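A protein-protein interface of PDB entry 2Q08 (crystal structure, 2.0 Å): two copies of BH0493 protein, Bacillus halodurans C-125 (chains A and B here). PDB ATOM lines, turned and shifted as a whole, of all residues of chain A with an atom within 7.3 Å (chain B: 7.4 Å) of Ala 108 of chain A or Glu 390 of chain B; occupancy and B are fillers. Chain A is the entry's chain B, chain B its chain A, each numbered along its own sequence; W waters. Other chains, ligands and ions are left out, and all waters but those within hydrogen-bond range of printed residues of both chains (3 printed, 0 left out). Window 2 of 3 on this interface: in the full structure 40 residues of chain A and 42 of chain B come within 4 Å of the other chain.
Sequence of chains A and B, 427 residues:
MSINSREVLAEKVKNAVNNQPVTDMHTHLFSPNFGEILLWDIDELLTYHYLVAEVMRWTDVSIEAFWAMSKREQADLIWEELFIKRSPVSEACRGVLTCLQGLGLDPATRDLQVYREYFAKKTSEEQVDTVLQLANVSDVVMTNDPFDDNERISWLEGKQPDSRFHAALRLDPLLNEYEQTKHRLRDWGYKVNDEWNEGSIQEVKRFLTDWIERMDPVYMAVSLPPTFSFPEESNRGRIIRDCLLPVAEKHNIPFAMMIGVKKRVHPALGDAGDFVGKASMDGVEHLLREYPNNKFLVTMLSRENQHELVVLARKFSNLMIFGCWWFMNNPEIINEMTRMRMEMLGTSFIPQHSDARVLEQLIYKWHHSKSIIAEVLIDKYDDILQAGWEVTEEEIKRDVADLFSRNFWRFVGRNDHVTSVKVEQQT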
ATOM      1  N   SER A  87     -19.469 -21.416 -16.621  1.00  0.00           N
ATOM      2  CA  SER A  87     -19.807 -21.579 -15.210  1.00  0.00           C
ATOM      3  C   SER A  87     -20.663 -22.825 -15.049  1.00  0.00           C
ATOM      4  O   SER A  87     -21.543 -23.094 -15.865  1.00  0.00           O
ATOM      5  CB  SER A  87     -20.550 -20.356 -14.706  1.00  0.00           C
ATOM      6  OG  SER A  87     -19.720 -19.217 -14.795  1.00  0.00           O
ATOM      7  N   PRO A  88     -20.396 -23.621 -14.008  1.00  0.00           N
ATOM      8  CA  PRO A  88     -21.136 -24.855 -13.725  1.00  0.00           C
ATOM      9  C   PRO A  88     -22.527 -24.599 -13.125  1.00  0.00           C
ATOM     10  O   PRO A  88     -22.824 -25.059 -12.024  1.00  0.00           O
ATOM     11  CB  PRO A  88     -20.214 -25.580 -12.752  1.00  0.00           C
ATOM     12  CG  PRO A  88     -19.634 -24.442 -11.947  1.00  0.00           C
ATOM     13  CD  PRO A  88     -19.332 -23.392 -13.006  1.00  0.00           C
ATOM     14  N   LEU A  97     -20.473 -29.730  -7.026  1.00  0.00           N
ATOM     15  CA  LEU A  97     -19.921 -28.754  -6.095  1.00  0.00           C
ATOM     16  C   LEU A  97     -20.480 -28.932  -4.684  1.00  0.00           C
ATOM     17  O   LEU A  97     -19.735 -28.865  -3.703  1.00  0.00           O
ATOM     18  CB  LEU A  97     -20.190 -27.332  -6.598  1.00  0.00           C
ATOM     19  CG  LEU A  97     -19.670 -27.077  -8.021  1.00  0.00           C
ATOM     20  CD1 LEU A  97     -19.955 -25.645  -8.431  1.00  0.00           C
ATOM     21  CD2 LEU A  97     -18.170 -27.351  -8.071  1.00  0.00           C
ATOM     22  N   LEU A 105     -14.283 -30.398   1.273  1.00  0.00           N
ATOM     23  CA  LEU A 105     -13.354 -29.961   0.240  1.00  0.00           C
ATOM     24  C   LEU A 105     -13.784 -28.559  -0.177  1.00  0.00           C
ATOM     25  O   LEU A 105     -14.929 -28.175   0.037  1.00  0.00           O
ATOM     26  CB  LEU A 105     -13.387 -30.928  -0.940  1.00  0.00           C
ATOM     27  CG  LEU A 105     -12.965 -32.350  -0.550  1.00  0.00           C
ATOM     28  CD1 LEU A 105     -13.116 -33.299  -1.726  1.00  0.00           C
ATOM     29  CD2 LEU A 105     -11.519 -32.328  -0.065  1.00  0.00           C
ATOM     30  N   ASP A 106     -12.879 -27.788  -0.764  1.00  0.00           N
ATOM     31  CA  ASP A 106     -13.207 -26.420  -1.130  1.00  0.00           C
ATOM     32  C   ASP A 106     -13.266 -26.133  -2.630  1.00  0.00           C
ATOM     33  O   ASP A 106     -12.237 -26.056  -3.303  1.00  0.00           O
ATOM     34  CB  ASP A 106     -12.218 -25.471  -0.445  1.00  0.00           C
ATOM     35  CG  ASP A 106     -12.504 -24.017  -0.738  1.00  0.00           C
ATOM     36  OD1 ASP A 106     -13.692 -23.654  -0.858  1.00  0.00           O
ATOM     37  OD2 ASP A 106     -11.541 -23.230  -0.838  1.00  0.00           O
ATOM     38  N   PRO A 107     -14.485 -25.960  -3.167  1.00  0.00           N
ATOM     39  CA  PRO A 107     -14.706 -25.680  -4.589  1.00  0.00           C
ATOM     40  C   PRO A 107     -14.055 -24.376  -5.036  1.00  0.00           C
ATOM     41  O   PRO A 107     -13.760 -24.186  -6.217  1.00  0.00           O
ATOM     42  CB  PRO A 107     -16.227 -25.621  -4.696  1.00  0.00           C
ATOM     43  CG  PRO A 107     -16.680 -26.544  -3.601  1.00  0.00           C
ATOM     44  CD  PRO A 107     -15.767 -26.152  -2.469  1.00  0.00           C
ATOM     45  N   ALA A 108     -13.833 -23.477  -4.085  1.00  0.00           N
ATOM     46  CA  ALA A 108     -13.225 -22.186  -4.383  1.00  0.00           C
ATOM     47  C   ALA A 108     -11.854 -22.316  -5.052  1.00  0.00           C
ATOM     48  O   ALA A 108     -11.477 -21.476  -5.874  1.00  0.00           O
ATOM     49  CB  ALA A 108     -13.103 -21.368  -3.108  1.00  0.00           C
ATOM     50  N   THR A 109     -11.116 -23.368  -4.708  1.00  0.00           N
ATOM     51  CA  THR A 109      -9.790 -23.577  -5.281  1.00  0.00           C
ATOM     52  C   THR A 109      -9.799 -24.235  -6.655  1.00  0.00           C
ATOM     53  O   THR A 109      -8.840 -24.094  -7.415  1.00  0.00           O
ATOM     54  CB  THR A 109      -8.913 -24.441  -4.366  1.00  0.00           C
ATOM     55  OG1 THR A 109      -9.482 -25.751  -4.255  1.00  0.00           O
ATOM     56  CG2 THR A 109      -8.813 -23.817  -2.987  1.00  0.00           C
ATOM     57  N   ARG A 110     -10.874 -24.958  -6.967  1.00  0.00           N
ATOM     58  CA  ARG A 110     -10.994 -25.647  -8.251  1.00  0.00           C
ATOM     59  C   ARG A 110      -9.826 -26.619  -8.423  1.00  0.00           C
ATOM     60  O   ARG A 110      -9.464 -26.975  -9.543  1.00  0.00           O
ATOM     61  CB  ARG A 110     -10.995 -24.637  -9.408  1.00  0.00           C
ATOM     62  CG  ARG A 110     -12.028 -23.526  -9.268  1.00  0.00           C
ATOM     63  CD  ARG A 110     -12.114 -22.670 -10.518  1.00  0.00           C
ATOM     64  NE  ARG A 110     -13.092 -21.592 -10.362  1.00  0.00           N
ATOM     65  CZ  ARG A 110     -13.435 -20.742 -11.330  1.00  0.00           C
ATOM     66  NH1 ARG A 110     -12.880 -20.838 -12.531  1.00  0.00           N
ATOM     67  NH2 ARG A 110     -14.343 -19.799 -11.100  1.00  0.00           N
ATOM     68  N   ASP A 111      -9.251 -27.046  -7.301  1.00  0.00           N
ATOM     69  CA  ASP A 111      -8.114 -27.966  -7.311  1.00  0.00           C
ATOM     70  C   ASP A 111      -8.567 -29.421  -7.361  1.00  0.00           C
ATOM     71  O   ASP A 111      -8.661 -30.089  -6.329  1.00  0.00           O
ATOM     72  CB  ASP A 111      -7.253 -27.751  -6.065  1.00  0.00           C
ATOM     73  CG  ASP A 111      -5.834 -28.270  -6.239  1.00  0.00           C
ATOM     74  OD1 ASP A 111      -5.656 -29.360  -6.824  1.00  0.00           O
ATOM     75  OD2 ASP A 111      -4.901 -27.581  -5.779  1.00  0.00           O
ATOM     76  N   TYR A 115      -8.794 -32.615  -4.546  1.00  0.00           N
ATOM     77  CA  TYR A 115     -10.054 -33.305  -4.269  1.00  0.00           C
ATOM     78  C   TYR A 115      -9.847 -34.811  -4.383  1.00  0.00           C
ATOM     79  O   TYR A 115     -10.313 -35.577  -3.541  1.00  0.00           O
ATOM     80  CB  TYR A 115     -11.168 -32.877  -5.245  1.00  0.00           C
ATOM     81  CG  TYR A 115     -11.414 -31.384  -5.330  1.00  0.00           C
ATOM     82  CD1 TYR A 115     -11.194 -30.550  -4.237  1.00  0.00           C
ATOM     83  CD2 TYR A 115     -11.861 -30.808  -6.515  1.00  0.00           C
ATOM     84  CE1 TYR A 115     -11.415 -29.170  -4.328  1.00  0.00           C
ATOM     85  CE2 TYR A 115     -12.084 -29.442  -6.618  1.00  0.00           C
ATOM     86  CZ  TYR A 115     -11.860 -28.629  -5.527  1.00  0.00           C
ATOM     87  OH  TYR A 115     -12.078 -27.273  -5.640  1.00  0.00           O
ATOM     88  N   SER B   2     -14.824  -8.580  -5.180  1.00  0.00           N
ATOM     89  CA  SER B   2     -15.304  -9.920  -4.877  1.00  0.00           C
ATOM     90  C   SER B   2     -16.818 -10.073  -4.937  1.00  0.00           C
ATOM     91  O   SER B   2     -17.560  -9.410  -4.199  1.00  0.00           O
ATOM     92  CB  SER B   2     -14.807 -10.350  -3.490  1.00  0.00           C
ATOM     93  OG  SER B   2     -15.253 -11.660  -3.163  1.00  0.00           O
ATOM     94  N   ILE B   3     -17.275 -10.946  -5.825  1.00  0.00           N
ATOM     95  CA  ILE B   3     -18.696 -11.208  -5.940  1.00  0.00           C
ATOM     96  C   ILE B   3     -18.909 -12.277  -4.876  1.00  0.00           C
ATOM     97  O   ILE B   3     -18.695 -13.463  -5.128  1.00  0.00           O
ATOM     98  CB  ILE B   3     -19.047 -11.747  -7.334  1.00  0.00           C
ATOM     99  CG1 ILE B   3     -18.561 -10.752  -8.393  1.00  0.00           C
ATOM    100  CG2 ILE B   3     -20.554 -11.961  -7.442  1.00  0.00           C
ATOM    101  CD1 ILE B   3     -18.872 -11.156  -9.833  1.00  0.00           C
ATOM    102  N   ILE B 384     -24.442 -21.805  -6.895  1.00  0.00           N
ATOM    103  CA  ILE B 384     -23.091 -22.381  -6.878  1.00  0.00           C
ATOM    104  C   ILE B 384     -22.160 -21.527  -6.016  1.00  0.00           C
ATOM    105  O   ILE B 384     -21.202 -22.033  -5.434  1.00  0.00           O
ATOM    106  CB  ILE B 384     -22.489 -22.580  -8.308  1.00  0.00           C
ATOM    107  CG1 ILE B 384     -22.469 -21.275  -9.094  1.00  0.00           C
ATOM    108  CG2 ILE B 384     -23.292 -23.634  -9.045  1.00  0.00           C
ATOM    109  CD1 ILE B 384     -21.807 -21.440 -10.489  1.00  0.00           C
ATOM    110  N   LEU B 385     -22.455 -20.237  -5.907  1.00  0.00           N
ATOM    111  CA  LEU B 385     -21.652 -19.376  -5.056  1.00  0.00           C
ATOM    112  C   LEU B 385     -21.824 -19.887  -3.626  1.00  0.00           C
ATOM    113  O   LEU B 385     -20.847 -20.042  -2.888  1.00  0.00           O
ATOM    114  CB  LEU B 385     -22.129 -17.915  -5.132  1.00  0.00           C
ATOM    115  CG  LEU B 385     -21.600 -16.995  -4.017  1.00  0.00           C
ATOM    116  CD1 LEU B 385     -20.078 -16.864  -4.132  1.00  0.00           C
ATOM    117  CD2 LEU B 385     -22.263 -15.614  -4.115  1.00  0.00           C
ATOM    118  N   ALA B 387     -22.445 -22.746  -2.741  1.00  0.00           N
ATOM    119  CA  ALA B 387     -21.838 -24.072  -2.616  1.00  0.00           C
ATOM    120  C   ALA B 387     -20.318 -23.941  -2.517  1.00  0.00           C
ATOM    121  O   ALA B 387     -19.611 -24.938  -2.391  1.00  0.00           O
ATOM    122  CB  ALA B 387     -22.210 -24.954  -3.796  1.00  0.00           C
ATOM    123  N   GLY B 388     -19.822 -22.708  -2.589  1.00  0.00           N
ATOM    124  CA  GLY B 388     -18.390 -22.483  -2.469  1.00  0.00           C
ATOM    125  C   GLY B 388     -17.652 -22.132  -3.748  1.00  0.00           C
ATOM    126  O   GLY B 388     -16.431 -21.940  -3.735  1.00  0.00           O
ATOM    127  N   TRP B 389     -18.374 -22.052  -4.857  1.00  0.00           N
ATOM    128  CA  TRP B 389     -17.748 -21.717  -6.131  1.00  0.00           C
ATOM    129  C   TRP B 389     -17.504 -20.224  -6.253  1.00  0.00           C
ATOM    130  O   TRP B 389     -18.344 -19.404  -5.866  1.00  0.00           O
ATOM    131  CB  TRP B 389     -18.632 -22.172  -7.291  1.00  0.00           C
ATOM    132  CG  TRP B 389     -17.992 -22.034  -8.656  1.00  0.00           C
ATOM    133  CD1 TRP B 389     -18.203 -21.042  -9.572  1.00  0.00           C
ATOM    134  CD2 TRP B 389     -17.085 -22.952  -9.264  1.00  0.00           C
ATOM    135  NE1 TRP B 389     -17.486 -21.293 -10.725  1.00  0.00           N
ATOM    136  CE2 TRP B 389     -16.790 -22.460 -10.559  1.00  0.00           C
ATOM    137  CE3 TRP B 389     -16.487 -24.145  -8.841  1.00  0.00           C
ATOM    138  CZ2 TRP B 389     -15.926 -23.125 -11.432  1.00  0.00           C
ATOM    139  CZ3 TRP B 389     -15.629 -24.804  -9.707  1.00  0.00           C
ATOM    140  CH2 TRP B 389     -15.356 -24.288 -10.991  1.00  0.00           C
ATOM    141  N   GLU B 390     -16.346 -19.858  -6.780  1.00  0.00           N
ATOM    142  CA  GLU B 390     -16.059 -18.447  -6.968  1.00  0.00           C
ATOM    143  C   GLU B 390     -16.369 -18.068  -8.410  1.00  0.00           C
ATOM    144  O   GLU B 390     -15.733 -18.563  -9.334  1.00  0.00           O
ATOM    145  CB  GLU B 390     -14.591 -18.138  -6.674  1.00  0.00           C
ATOM    146  CG  GLU B 390     -14.238 -18.169  -5.204  1.00  0.00           C
ATOM    147  CD  GLU B 390     -12.871 -17.573  -4.925  1.00  0.00           C
ATOM    148  OE1 GLU B 390     -12.496 -17.493  -3.736  1.00  0.00           O
ATOM    149  OE2 GLU B 390     -12.178 -17.184  -5.894  1.00  0.00           O
ATOM    150  N   VAL B 391     -17.351 -17.199  -8.607  1.00  0.00           N
ATOM    151  CA  VAL B 391     -17.689 -16.758  -9.949  1.00  0.00           C
ATOM    152  C   VAL B 391     -17.113 -15.355 -10.135  1.00  0.00           C
ATOM    153  O   VAL B 391     -17.347 -14.464  -9.314  1.00  0.00           O
ATOM    154  CB  VAL B 391     -19.225 -16.739 -10.169  1.00  0.00           C
ATOM    155  CG1 VAL B 391     -19.881 -15.868  -9.140  1.00  0.00           C
ATOM    156  CG2 VAL B 391     -19.549 -16.234 -11.568  1.00  0.00           C
ATOM    157  N   THR B 392     -16.335 -15.165 -11.195  1.00  0.00           N
ATOM    158  CA  THR B 392     -15.736 -13.858 -11.460  1.00  0.00           C
ATOM    159  C   THR B 392     -16.631 -13.087 -12.416  1.00  0.00           C
ATOM    160  O   THR B 392     -17.434 -13.680 -13.147  1.00  0.00           O
ATOM    161  CB  THR B 392     -14.342 -13.992 -12.102  1.00  0.00           C
ATOM    162  OG1 THR B 392     -14.482 -14.504 -13.432  1.00  0.00           O
ATOM    163  CG2 THR B 392     -13.471 -14.944 -11.294  1.00  0.00           C
ATOM    164  N   GLU B 395     -16.213 -14.175 -15.927  1.00  0.00           N
ATOM    165  CA  GLU B 395     -16.876 -15.428 -16.268  1.00  0.00           C
ATOM    166  C   GLU B 395     -18.359 -15.165 -16.526  1.00  0.00           C
ATOM    167  O   GLU B 395     -18.942 -15.772 -17.422  1.00  0.00           O
ATOM    168  CB  GLU B 395     -16.681 -16.472 -15.150  1.00  0.00           C
ATOM    169  CG  GLU B 395     -15.209 -16.882 -14.978  1.00  0.00           C
ATOM    170  CD  GLU B 395     -14.954 -17.808 -13.799  1.00  0.00           C
ATOM    171  OE1 GLU B 395     -15.675 -17.725 -12.778  1.00  0.00           O
ATOM    172  OE2 GLU B 395     -14.006 -18.612 -13.885  1.00  0.00           O
HETATM  173  O   HOH W   1     -14.155 -21.500  -7.781  1.00  0.00           O
HETATM  174  O   HOH W   2     -12.808 -19.861 -15.882  1.00  0.00           O
HETATM  175  O   HOH W   3     -17.575 -19.535 -13.065  1.00  0.00           O
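Among the printed residues, merely in contact across the chains: Pro 88 of chain A with Ile 384 of chain B, Arg 110 of chain A with Trp 389 of chain B, Pro 107 of chain A with Ala 387 of chain B, Pro 88 of chain A with Trp 389 of chain B, Pro 107 of chain A with Gly 388 of chain B, Leu 97 of chain A with Trp 389 of chain B, Pro 107 of chain A with Trp 389 of chain B, Leu 97 of chain A with Ile 384 of chain B and Ala 108 of chain A with Glu 390 of chain B.
Printed residues of chain A that touch a printed residue of chain B: Pro 88, Leu 97, Pro 107, Ala 108 and Arg 110. Hydrophobic or aromatic side chains of chain A within 4 Å of the printed part of chain B: Pro 88, Leu 97, Pro 107 and Ala 108. Of the 11 printed residues of chain B, 6 touch a printed residue of chain A. Printed residues of chain B that touch a printed residue of chain A: Ile 384, Ala 387, Gly 388, Trp 389, Glu 390 and Glu 395. Among the printed residues, 12 pairs touch across the chains. Among the printed residues, Asp or Glu carboxylates within 4 Å of a Lys or Arg side-chain nitrogen of the other chain: Arg 110 of chain A with Glu 395 of chain B (2.8 Å).
O of Gly 388 of chain B sits at hydrogen-bond distance from N of Ala 108 of chain A (3.0 Å). The guanidinium group of Arg 110 of chain A sits at hydrogen-bond distance from the backbone carbonyl oxygen of Glu 390 of chain B (2.6 Å). The side-chain carboxylate of Glu 395 of chain B lies within salt-bridge range of the guanidinium group of Arg 110 of chain A (2.8 Å).
Water W3 lies within hydrogen-bond range of the side-chain carboxylate of Glu 395 of chain B (2.6 Å), the side-chain hydroxyl of Ser 87 of chain A (2.8 Å) and the indole nitrogen of Trp 389 of chain B (2.9 Å). Water W2 lies within hydrogen-bond range of the side-chain carboxylate of Glu 395 of chain B (2.6 Å) and the guanidinium group of Arg 110 of chain A (3.5 Å). Water W1 lies within hydrogen-bond range of the guanidinium group (NE) of Arg 110 of chain A (2.8 Å), the backbone NH (N) of Glu 390 of chain B (2.9 Å), the backbone carbonyl oxygen (O) of Pro 107 of chain A (3.1 Å) and the backbone carbonyl oxygen (O) of Ala 108 of chain A (3.3 Å).
O of Ile 384 of chain B lies within hydrogen-bond range of N of Trp 389 of chain B. The side-chain hydroxyl of Thr 392 of chain B sits close to the backbone NH of Glu 395 of chain B (3.1 Å). N of Ala 108 of chain A lies close to OD1 of Asp 106 of chain A (3.2 Å). The backbone NH (N) of Arg 110 of chain A sits at hydrogen-bond distance from the side-chain hydroxyl (OH) of Tyr 115 of chain A (2.9 Å).
Printed residues of chain B within 4 Å of Pro 88 of chain A: Ile 384 (3.3 Å) and Trp 389 (3.6 Å). Of the printed residues of chain B, Leu 97 of chain A touches Ile 384 and Trp 389. Ala 108 of chain A touches two residues of chain B. Of the printed residues of chain B, Arg 110 of chain A touches Trp 389 (3.4 Å), Glu 390 (2.6 Å) and Glu 395 (2.8 Å). The nearest residue of chain B that does not touch Ala 108 of chain A is Trp 389 of chain B (4.8 Å). The nearest residue of chain A that does not touch Glu 390 of chain B is Pro 107 of chain A (5.1 Å).
No position is printed for both chains.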
